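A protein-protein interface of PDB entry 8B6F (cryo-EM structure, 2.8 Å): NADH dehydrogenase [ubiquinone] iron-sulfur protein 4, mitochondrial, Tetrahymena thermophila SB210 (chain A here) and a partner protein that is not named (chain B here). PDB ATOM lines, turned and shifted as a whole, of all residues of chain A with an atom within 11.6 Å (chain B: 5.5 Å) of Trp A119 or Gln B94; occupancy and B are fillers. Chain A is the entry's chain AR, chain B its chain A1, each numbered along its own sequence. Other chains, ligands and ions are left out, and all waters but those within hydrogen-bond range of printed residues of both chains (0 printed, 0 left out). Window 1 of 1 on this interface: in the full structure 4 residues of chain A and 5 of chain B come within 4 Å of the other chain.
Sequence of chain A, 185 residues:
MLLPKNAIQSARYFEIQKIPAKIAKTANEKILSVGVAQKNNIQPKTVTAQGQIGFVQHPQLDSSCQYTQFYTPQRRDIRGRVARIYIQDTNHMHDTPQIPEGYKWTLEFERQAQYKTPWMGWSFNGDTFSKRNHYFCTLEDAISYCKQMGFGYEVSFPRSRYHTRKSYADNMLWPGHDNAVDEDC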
ATOM      1  N   TYR A 115      29.646  15.774   6.173  1.00  0.00           N
ATOM      2  CA  TYR A 115      28.717  14.960   5.407  1.00  0.00           C
ATOM      3  C   TYR A 115      29.195  14.830   3.969  1.00  0.00           C
ATOM      4  O   TYR A 115      29.807  15.747   3.417  1.00  0.00           O
ATOM      5  CB  TYR A 115      27.304  15.558   5.432  1.00  0.00           C
ATOM      6  CG  TYR A 115      27.268  17.044   5.158  1.00  0.00           C
ATOM      7  CD1 TYR A 115      27.448  17.962   6.184  1.00  0.00           C
ATOM      8  CD2 TYR A 115      27.045  17.527   3.877  1.00  0.00           C
ATOM      9  CE1 TYR A 115      27.416  19.319   5.940  1.00  0.00           C
ATOM     10  CE2 TYR A 115      27.010  18.882   3.623  1.00  0.00           C
ATOM     11  CZ  TYR A 115      27.195  19.773   4.659  1.00  0.00           C
ATOM     12  OH  TYR A 115      27.160  21.124   4.410  1.00  0.00           O
ATOM     13  N   LYS A 116      28.917  13.676   3.372  1.00  0.00           N
ATOM     14  CA  LYS A 116      29.257  13.423   1.980  1.00  0.00           C
ATOM     15  C   LYS A 116      28.049  13.760   1.114  1.00  0.00           C
ATOM     16  O   LYS A 116      26.975  13.174   1.285  1.00  0.00           O
ATOM     17  CB  LYS A 116      29.683  11.970   1.780  1.00  0.00           C
ATOM     18  CG  LYS A 116      30.884  11.570   2.620  1.00  0.00           C
ATOM     19  CD  LYS A 116      31.231  10.099   2.448  1.00  0.00           C
ATOM     20  CE  LYS A 116      31.856   9.814   1.095  1.00  0.00           C
ATOM     21  NZ  LYS A 116      33.139  10.544   0.905  1.00  0.00           N
ATOM     22  N   THR A 117      28.225  14.698   0.190  1.00  0.00           N
ATOM     23  CA  THR A 117      27.122  15.149  -0.636  1.00  0.00           C
ATOM     24  C   THR A 117      26.700  14.044  -1.604  1.00  0.00           C
ATOM     25  O   THR A 117      27.498  13.172  -1.946  1.00  0.00           O
ATOM     26  CB  THR A 117      27.512  16.405  -1.403  1.00  0.00           C
ATOM     27  OG1 THR A 117      28.727  16.172  -2.126  1.00  0.00           O
ATOM     28  CG2 THR A 117      27.697  17.563  -0.442  1.00  0.00           C
ATOM     29  N   PRO A 118      25.445  14.061  -2.063  1.00  0.00           N
ATOM     30  CA  PRO A 118      24.958  12.943  -2.885  1.00  0.00           C
ATOM     31  C   PRO A 118      25.482  12.951  -4.315  1.00  0.00           C
ATOM     32  O   PRO A 118      25.731  11.883  -4.881  1.00  0.00           O
ATOM     33  CB  PRO A 118      23.432  13.123  -2.860  1.00  0.00           C
ATOM     34  CG  PRO A 118      23.155  14.175  -1.830  1.00  0.00           C
ATOM     35  CD  PRO A 118      24.370  15.025  -1.776  1.00  0.00           C
ATOM     36  N   TRP A 119      25.653  14.132  -4.912  1.00  0.00           N
ATOM     37  CA  TRP A 119      25.911  14.189  -6.350  1.00  0.00           C
ATOM     38  C   TRP A 119      27.226  13.511  -6.715  1.00  0.00           C
ATOM     39  O   TRP A 119      27.315  12.836  -7.747  1.00  0.00           O
ATOM     40  CB  TRP A 119      25.900  15.639  -6.838  1.00  0.00           C
ATOM     41  CG  TRP A 119      26.802  16.566  -6.087  1.00  0.00           C
ATOM     42  CD1 TRP A 119      28.138  16.752  -6.284  1.00  0.00           C
ATOM     43  CD2 TRP A 119      26.424  17.454  -5.029  1.00  0.00           C
ATOM     44  NE1 TRP A 119      28.617  17.697  -5.409  1.00  0.00           N
ATOM     45  CE2 TRP A 119      27.584  18.142  -4.628  1.00  0.00           C
ATOM     46  CE3 TRP A 119      25.217  17.728  -4.380  1.00  0.00           C
ATOM     47  CZ2 TRP A 119      27.574  19.087  -3.606  1.00  0.00           C
ATOM     48  CZ3 TRP A 119      25.207  18.667  -3.366  1.00  0.00           C
ATOM     49  CH2 TRP A 119      26.379  19.337  -2.988  1.00  0.00           C
ATOM     50  N   MET A 120      28.262  13.680  -5.892  1.00  0.00           N
ATOM     51  CA  MET A 120      29.566  13.100  -6.175  1.00  0.00           C
ATOM     52  C   MET A 120      30.200  12.402  -4.981  1.00  0.00           C
ATOM     53  O   MET A 120      31.283  11.826  -5.130  1.00  0.00           O
ATOM     54  CB  MET A 120      30.533  14.180  -6.686  1.00  0.00           C
ATOM     55  CG  MET A 120      30.315  14.577  -8.137  1.00  0.00           C
ATOM     56  SD  MET A 120      30.820  13.292  -9.298  1.00  0.00           S
ATOM     57  CE  MET A 120      32.602  13.374  -9.160  1.00  0.00           C
ATOM     58  N   GLY A 121      29.566  12.423  -3.812  1.00  0.00           N
ATOM     59  CA  GLY A 121      30.165  11.810  -2.645  1.00  0.00           C
ATOM     60  C   GLY A 121      31.324  12.580  -2.061  1.00  0.00           C
ATOM     61  O   GLY A 121      32.146  12.000  -1.350  1.00  0.00           O
ATOM     62  N   TRP A 122      31.418  13.874  -2.350  1.00  0.00           N
ATOM     63  CA  TRP A 122      32.495  14.700  -1.825  1.00  0.00           C
ATOM     64  C   TRP A 122      32.194  15.127  -0.395  1.00  0.00           C
ATOM     65  O   TRP A 122      31.045  15.400  -0.039  1.00  0.00           O
ATOM     66  CB  TRP A 122      32.698  15.930  -2.709  1.00  0.00           C
ATOM     67  CG  TRP A 122      33.143  15.600  -4.100  1.00  0.00           C
ATOM     68  CD1 TRP A 122      33.715  14.436  -4.522  1.00  0.00           C
ATOM     69  CD2 TRP A 122      33.048  16.442  -5.254  1.00  0.00           C
ATOM     70  NE1 TRP A 122      33.985  14.502  -5.866  1.00  0.00           N
ATOM     71  CE2 TRP A 122      33.587  15.724  -6.339  1.00  0.00           C
ATOM     72  CE3 TRP A 122      32.564  17.735  -5.475  1.00  0.00           C
ATOM     73  CZ2 TRP A 122      33.652  16.253  -7.625  1.00  0.00           C
ATOM     74  CZ3 TRP A 122      32.630  18.260  -6.753  1.00  0.00           C
ATOM     75  CH2 TRP A 122      33.171  17.521  -7.812  1.00  0.00           C
ATOM     76  N   SER A 123      33.239  15.183   0.427  1.00  0.00           N
ATOM     77  CA  SER A 123      33.087  15.559   1.825  1.00  0.00           C
ATOM     78  C   SER A 123      32.916  17.066   1.954  1.00  0.00           C
ATOM     79  O   SER A 123      33.594  17.845   1.279  1.00  0.00           O
ATOM     80  CB  SER A 123      34.296  15.100   2.638  1.00  0.00           C
ATOM     81  OG  SER A 123      34.432  13.692   2.594  1.00  0.00           O
ATOM     82  N   PHE A 124      32.004  17.469   2.833  1.00  0.00           N
ATOM     83  CA  PHE A 124      31.698  18.866   3.095  1.00  0.00           C
ATOM     84  C   PHE A 124      31.658  19.094   4.597  1.00  0.00           C
ATOM     85  O   PHE A 124      31.194  18.233   5.350  1.00  0.00           O
ATOM     86  CB  PHE A 124      30.351  19.276   2.486  1.00  0.00           C
ATOM     87  CG  PHE A 124      30.403  19.560   1.010  1.00  0.00           C
ATOM     88  CD1 PHE A 124      30.762  18.576   0.109  1.00  0.00           C
ATOM     89  CD2 PHE A 124      30.049  20.808   0.525  1.00  0.00           C
ATOM     90  CE1 PHE A 124      30.794  18.835  -1.247  1.00  0.00           C
ATOM     91  CE2 PHE A 124      30.077  21.074  -0.828  1.00  0.00           C
ATOM     92  CZ  PHE A 124      30.447  20.084  -1.716  1.00  0.00           C
ATOM     93  N   ASN A 125      32.147  20.252   5.027  1.00  0.00           N
ATOM     94  CA  ASN A 125      32.152  20.638   6.430  1.00  0.00           C
ATOM     95  C   ASN A 125      31.103  21.715   6.658  1.00  0.00           C
ATOM     96  O   ASN A 125      31.044  22.697   5.910  1.00  0.00           O
ATOM     97  CB  ASN A 125      33.527  21.153   6.855  1.00  0.00           C
ATOM     98  CG  ASN A 125      34.633  20.159   6.577  1.00  0.00           C
ATOM     99  OD1 ASN A 125      34.401  18.953   6.514  1.00  0.00           O
ATOM    100  ND2 ASN A 125      35.851  20.661   6.415  1.00  0.00           N
ATOM    101  N   GLY A 126      30.276  21.530   7.687  1.00  0.00           N
ATOM    102  CA  GLY A 126      29.294  22.548   8.019  1.00  0.00           C
ATOM    103  C   GLY A 126      29.937  23.860   8.421  1.00  0.00           C
ATOM    104  O   GLY A 126      29.442  24.936   8.080  1.00  0.00           O
ATOM    105  N   ARG B  37      22.554  26.228   1.300  1.00  0.00           N
ATOM    106  CA  ARG B  37      22.384  25.521   0.034  1.00  0.00           C
ATOM    107  C   ARG B  37      23.267  24.284  -0.058  1.00  0.00           C
ATOM    108  O   ARG B  37      22.879  23.295  -0.689  1.00  0.00           O
ATOM    109  CB  ARG B  37      22.680  26.461  -1.134  1.00  0.00           C
ATOM    110  CG  ARG B  37      21.762  27.667  -1.196  1.00  0.00           C
ATOM    111  CD  ARG B  37      22.495  28.944  -0.849  1.00  0.00           C
ATOM    112  NE  ARG B  37      21.621  30.108  -0.922  1.00  0.00           N
ATOM    113  CZ  ARG B  37      21.264  30.709  -2.049  1.00  0.00           C
ATOM    114  NH1 ARG B  37      21.665  30.263  -3.227  1.00  0.00           N
ATOM    115  NH2 ARG B  37      20.486  31.785  -1.991  1.00  0.00           N
ATOM    116  N   GLN B  38      24.448  24.317   0.548  1.00  0.00           N
ATOM    117  CA  GLN B  38      25.393  23.213   0.450  1.00  0.00           C
ATOM    118  C   GLN B  38      25.147  22.121   1.482  1.00  0.00           C
ATOM    119  O   GLN B  38      25.886  21.131   1.499  1.00  0.00           O
ATOM    120  CB  GLN B  38      26.826  23.736   0.588  1.00  0.00           C
ATOM    121  CG  GLN B  38      27.220  24.736  -0.487  1.00  0.00           C
ATOM    122  CD  GLN B  38      27.086  24.172  -1.887  1.00  0.00           C
ATOM    123  OE1 GLN B  38      27.114  22.959  -2.086  1.00  0.00           O
ATOM    124  NE2 GLN B  38      26.931  25.054  -2.867  1.00  0.00           N
ATOM    125  N   SER B  39      24.148  22.276   2.343  1.00  0.00           N
ATOM    126  CA  SER B  39      23.812  21.245   3.312  1.00  0.00           C
ATOM    127  C   SER B  39      22.947  20.171   2.654  1.00  0.00           C
ATOM    128  O   SER B  39      22.596  20.252   1.474  1.00  0.00           O
ATOM    129  CB  SER B  39      23.105  21.863   4.515  1.00  0.00           C
ATOM    130  OG  SER B  39      22.804  20.880   5.490  1.00  0.00           O
ATOM    131  N   GLY B  63      15.220  24.453  -2.132  1.00  0.00           N
ATOM    132  CA  GLY B  63      16.614  24.342  -2.529  1.00  0.00           C
ATOM    133  C   GLY B  63      17.566  25.023  -1.566  1.00  0.00           C
ATOM    134  O   GLY B  63      18.667  24.526  -1.314  1.00  0.00           O
ATOM    135  N   GLY B  66      19.210  22.993   1.061  1.00  0.00           N
ATOM    136  CA  GLY B  66      19.972  21.844   0.624  1.00  0.00           C
ATOM    137  C   GLY B  66      19.170  20.729  -0.005  1.00  0.00           C
ATOM    138  O   GLY B  66      19.742  19.679  -0.311  1.00  0.00           O
ATOM    139  N   SER B  67      17.871  20.920  -0.210  1.00  0.00           N
ATOM    140  CA  SER B  67      17.043  19.868  -0.775  1.00  0.00           C
ATOM    141  C   SER B  67      17.339  19.678  -2.258  1.00  0.00           C
ATOM    142  O   SER B  67      17.740  20.607  -2.962  1.00  0.00           O
ATOM    143  CB  SER B  67      15.564  20.200  -0.588  1.00  0.00           C
ATOM    144  OG  SER B  67      15.277  20.483   0.770  1.00  0.00           O
ATOM    145  N   ASP B  68      17.134  18.452  -2.730  1.00  0.00           N
ATOM    146  CA  ASP B  68      17.253  18.154  -4.148  1.00  0.00           C
ATOM    147  C   ASP B  68      15.938  18.488  -4.837  1.00  0.00           C
ATOM    148  O   ASP B  68      14.866  18.103  -4.361  1.00  0.00           O
ATOM    149  CB  ASP B  68      17.609  16.684  -4.362  1.00  0.00           C
ATOM    150  CG  ASP B  68      18.916  16.301  -3.696  1.00  0.00           C
ATOM    151  OD1 ASP B  68      19.786  17.182  -3.539  1.00  0.00           O
ATOM    152  OD2 ASP B  68      19.075  15.116  -3.332  1.00  0.00           O
ATOM    153  N   VAL B  69      16.018  19.198  -5.959  1.00  0.00           N
ATOM    154  CA  VAL B  69      14.838  19.688  -6.661  1.00  0.00           C
ATOM    155  C   VAL B  69      14.907  19.230  -8.110  1.00  0.00           C
ATOM    156  O   VAL B  69      15.945  19.371  -8.764  1.00  0.00           O
ATOM    157  CB  VAL B  69      14.717  21.222  -6.577  1.00  0.00           C
ATOM    158  CG1 VAL B  69      14.505  21.658  -5.138  1.00  0.00           C
ATOM    159  CG2 VAL B  69      15.947  21.898  -7.158  1.00  0.00           C
ATOM    160  N   ILE B  70      13.804  18.671  -8.599  1.00  0.00           N
ATOM    161  CA  ILE B  70      13.643  18.292  -9.995  1.00  0.00           C
ATOM    162  C   ILE B  70      12.541  19.161 -10.579  1.00  0.00           C
ATOM    163  O   ILE B  70      11.503  19.368  -9.940  1.00  0.00           O
ATOM    164  CB  ILE B  70      13.293  16.797 -10.154  1.00  0.00           C
ATOM    165  CG1 ILE B  70      14.209  15.923  -9.290  1.00  0.00           C
ATOM    166  CG2 ILE B  70      13.367  16.389 -11.615  1.00  0.00           C
ATOM    167  CD1 ILE B  70      15.675  16.049  -9.611  1.00  0.00           C
ATOM    168  N   ALA B  90      18.602  25.510  -6.303  1.00  0.00           N
ATOM    169  CA  ALA B  90      19.397  24.697  -5.390  1.00  0.00           C
ATOM    170  C   ALA B  90      20.893  24.859  -5.626  1.00  0.00           C
ATOM    171  O   ALA B  90      21.631  25.208  -4.700  1.00  0.00           O
ATOM    172  CB  ALA B  90      19.001  23.221  -5.519  1.00  0.00           C
ATOM    173  N   GLY B  91      21.362  24.615  -6.841  1.00  0.00           N
ATOM    174  CA  GLY B  91      22.763  24.719  -7.169  1.00  0.00           C
ATOM    175  C   GLY B  91      23.190  23.558  -8.037  1.00  0.00           C
ATOM    176  O   GLY B  91      22.361  22.855  -8.612  1.00  0.00           O
ATOM    177  N   SER B  92      24.502  23.362  -8.124  1.00  0.00           N
ATOM    178  CA  SER B  92      25.060  22.306  -8.956  1.00  0.00           C
ATOM    179  C   SER B  92      25.001  20.971  -8.229  1.00  0.00           C
ATOM    180  O   SER B  92      25.469  20.849  -7.093  1.00  0.00           O
ATOM    181  CB  SER B  92      26.501  22.639  -9.333  1.00  0.00           C
ATOM    182  OG  SER B  92      27.311  22.779  -8.181  1.00  0.00           O
ATOM    183  N   GLY B  93      24.431  19.967  -8.892  1.00  0.00           N
ATOM    184  CA  GLY B  93      24.269  18.655  -8.314  1.00  0.00           C
ATOM    185  C   GLY B  93      23.027  18.490  -7.471  1.00  0.00           C
ATOM    186  O   GLY B  93      22.749  17.371  -7.019  1.00  0.00           O
ATOM    187  N   GLN B  94      22.266  19.560  -7.250  1.00  0.00           N
ATOM    188  CA  GLN B  94      21.038  19.506  -6.471  1.00  0.00           C
ATOM    189  C   GLN B  94      19.799  19.868  -7.272  1.00  0.00           C
ATOM    190  O   GLN B  94      18.730  19.324  -6.996  1.00  0.00           O
ATOM    191  CB  GLN B  94      21.138  20.445  -5.261  1.00  0.00           C
ATOM    192  CG  GLN B  94      22.213  20.043  -4.265  1.00  0.00           C
ATOM    193  CD  GLN B  94      22.394  21.063  -3.163  1.00  0.00           C
ATOM    194  OE1 GLN B  94      22.164  22.254  -3.359  1.00  0.00           O
ATOM    195  NE2 GLN B  94      22.802  20.598  -1.989  1.00  0.00           N
ATOM    196  N   SER B  95      19.910  20.767  -8.245  1.00  0.00           N
ATOM    197  CA  SER B  95      18.792  21.146  -9.099  1.00  0.00           C
ATOM    198  C   SER B  95      18.949  20.478 -10.457  1.00  0.00           C
ATOM    199  O   SER B  95      20.029  20.521 -11.054  1.00  0.00           O
ATOM    200  CB  SER B  95      18.707  22.664  -9.265  1.00  0.00           C
ATOM    201  OG  SER B  95      19.949  23.207  -9.675  1.00  0.00           O
ATOM    202  N   TYR B  96      17.875  19.857 -10.935  1.00  0.00           N
ATOM    203  CA  TYR B  96      17.855  19.208 -12.237  1.00  0.00           C
ATOM    204  C   TYR B  96      16.646  19.691 -13.021  1.00  0.00           C
ATOM    205  O   TYR B  96      15.577  19.922 -12.449  1.00  0.00           O
ATOM    206  CB  TYR B  96      17.821  17.681 -12.095  1.00  0.00           C
ATOM    207  CG  TYR B  96      17.638  16.945 -13.403  1.00  0.00           C
ATOM    208  CD1 TYR B  96      18.557  17.079 -14.434  1.00  0.00           C
ATOM    209  CD2 TYR B  96      16.554  16.100 -13.596  1.00  0.00           C
ATOM    210  CE1 TYR B  96      18.393  16.403 -15.627  1.00  0.00           C
ATOM    211  CE2 TYR B  96      16.382  15.420 -14.784  1.00  0.00           C
ATOM    212  CZ  TYR B  96      17.303  15.574 -15.795  1.00  0.00           C
ATOM    213  OH  TYR B  96      17.133  14.894 -16.979  1.00  0.00           O
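Among the printed residues, merely in contact across the chains: Trp A119 with Gln B94, Tyr A115 with Ser B39, Trp A119 with Gly B93, Phe A124 with Gln B38 and Trp A119 with Gln B38.
Of the 16 printed residues of chain B, 4 touch a printed residue of chain A.
Printed residues of chain B that touch a printed residue of chain A: Gln B38, Ser B39, Gly B93 and Gln B94.
Hydrophobic or aromatic side chains of chain A within 4 Å of the printed part of chain B: Tyr A115, Trp A119 and Phe A124.
Among the printed residues, 6 pairs touch across the chains.
Of chain B, only Gln B38 (3.8 Å), Gly B93 (3.6 Å) and Gln B94 (3.4 Å) come within 4 Å of Trp A119.
Gln B94 touches just one residue of chain A: Trp A119.
Printed residues of chain A within 4 Å of Gln B38: Tyr A115, Trp A119 and Phe A124.
Ser B39 touches just one residue of chain A: Tyr A115 (3.5 Å).
No residue of chain A comes within 4 Å of Gly B66.
Val B69 touches none of the printed residues of chain A.
No residue of chain A comes within 4 Å of Ala B90.
No residue of chain A comes within 4 Å of Gly B91.
No residue of chain A comes within 4 Å of Ser B92.
Of chain A, only Trp A119 (3.6 Å) comes within 4 Å of Gly B93.
No residue of chain A comes within 4 Å of Ser B95.
Of the printed residues of chain B, Phe A124 touches Gln B38.
Printed residues of chain B within 4 Å of Tyr A115: Gln B38 and Ser B39.
The nearest residue of chain B that does not touch Trp A119 is Ser B92 (4.1 Å).
The backbone carbonyl oxygen of Gln B38 lies within hydrogen-bond range of the side-chain hydroxyl of Tyr A115, 3.2 Å away.
OE1 of Gln B94 sits close to O of Arg B37, at 3.0 Å.
NE2 of Gln B94 sits at hydrogen-bond distance from O of Ser B39 (3.5 Å).
The backbone NH (N) of Val B69 sits at hydrogen-bond distance from the backbone carbonyl oxygen (O) of Gln B94, 2.9 Å away.
The backbone carbonyl oxygen (O) of Ala B90 sits close to the side-chain amide oxygen (OE1) of Gln B94 (3.3 Å).
N of Phe A124 sits at hydrogen-bond distance from O of Tyr A115, 2.9 Å away.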
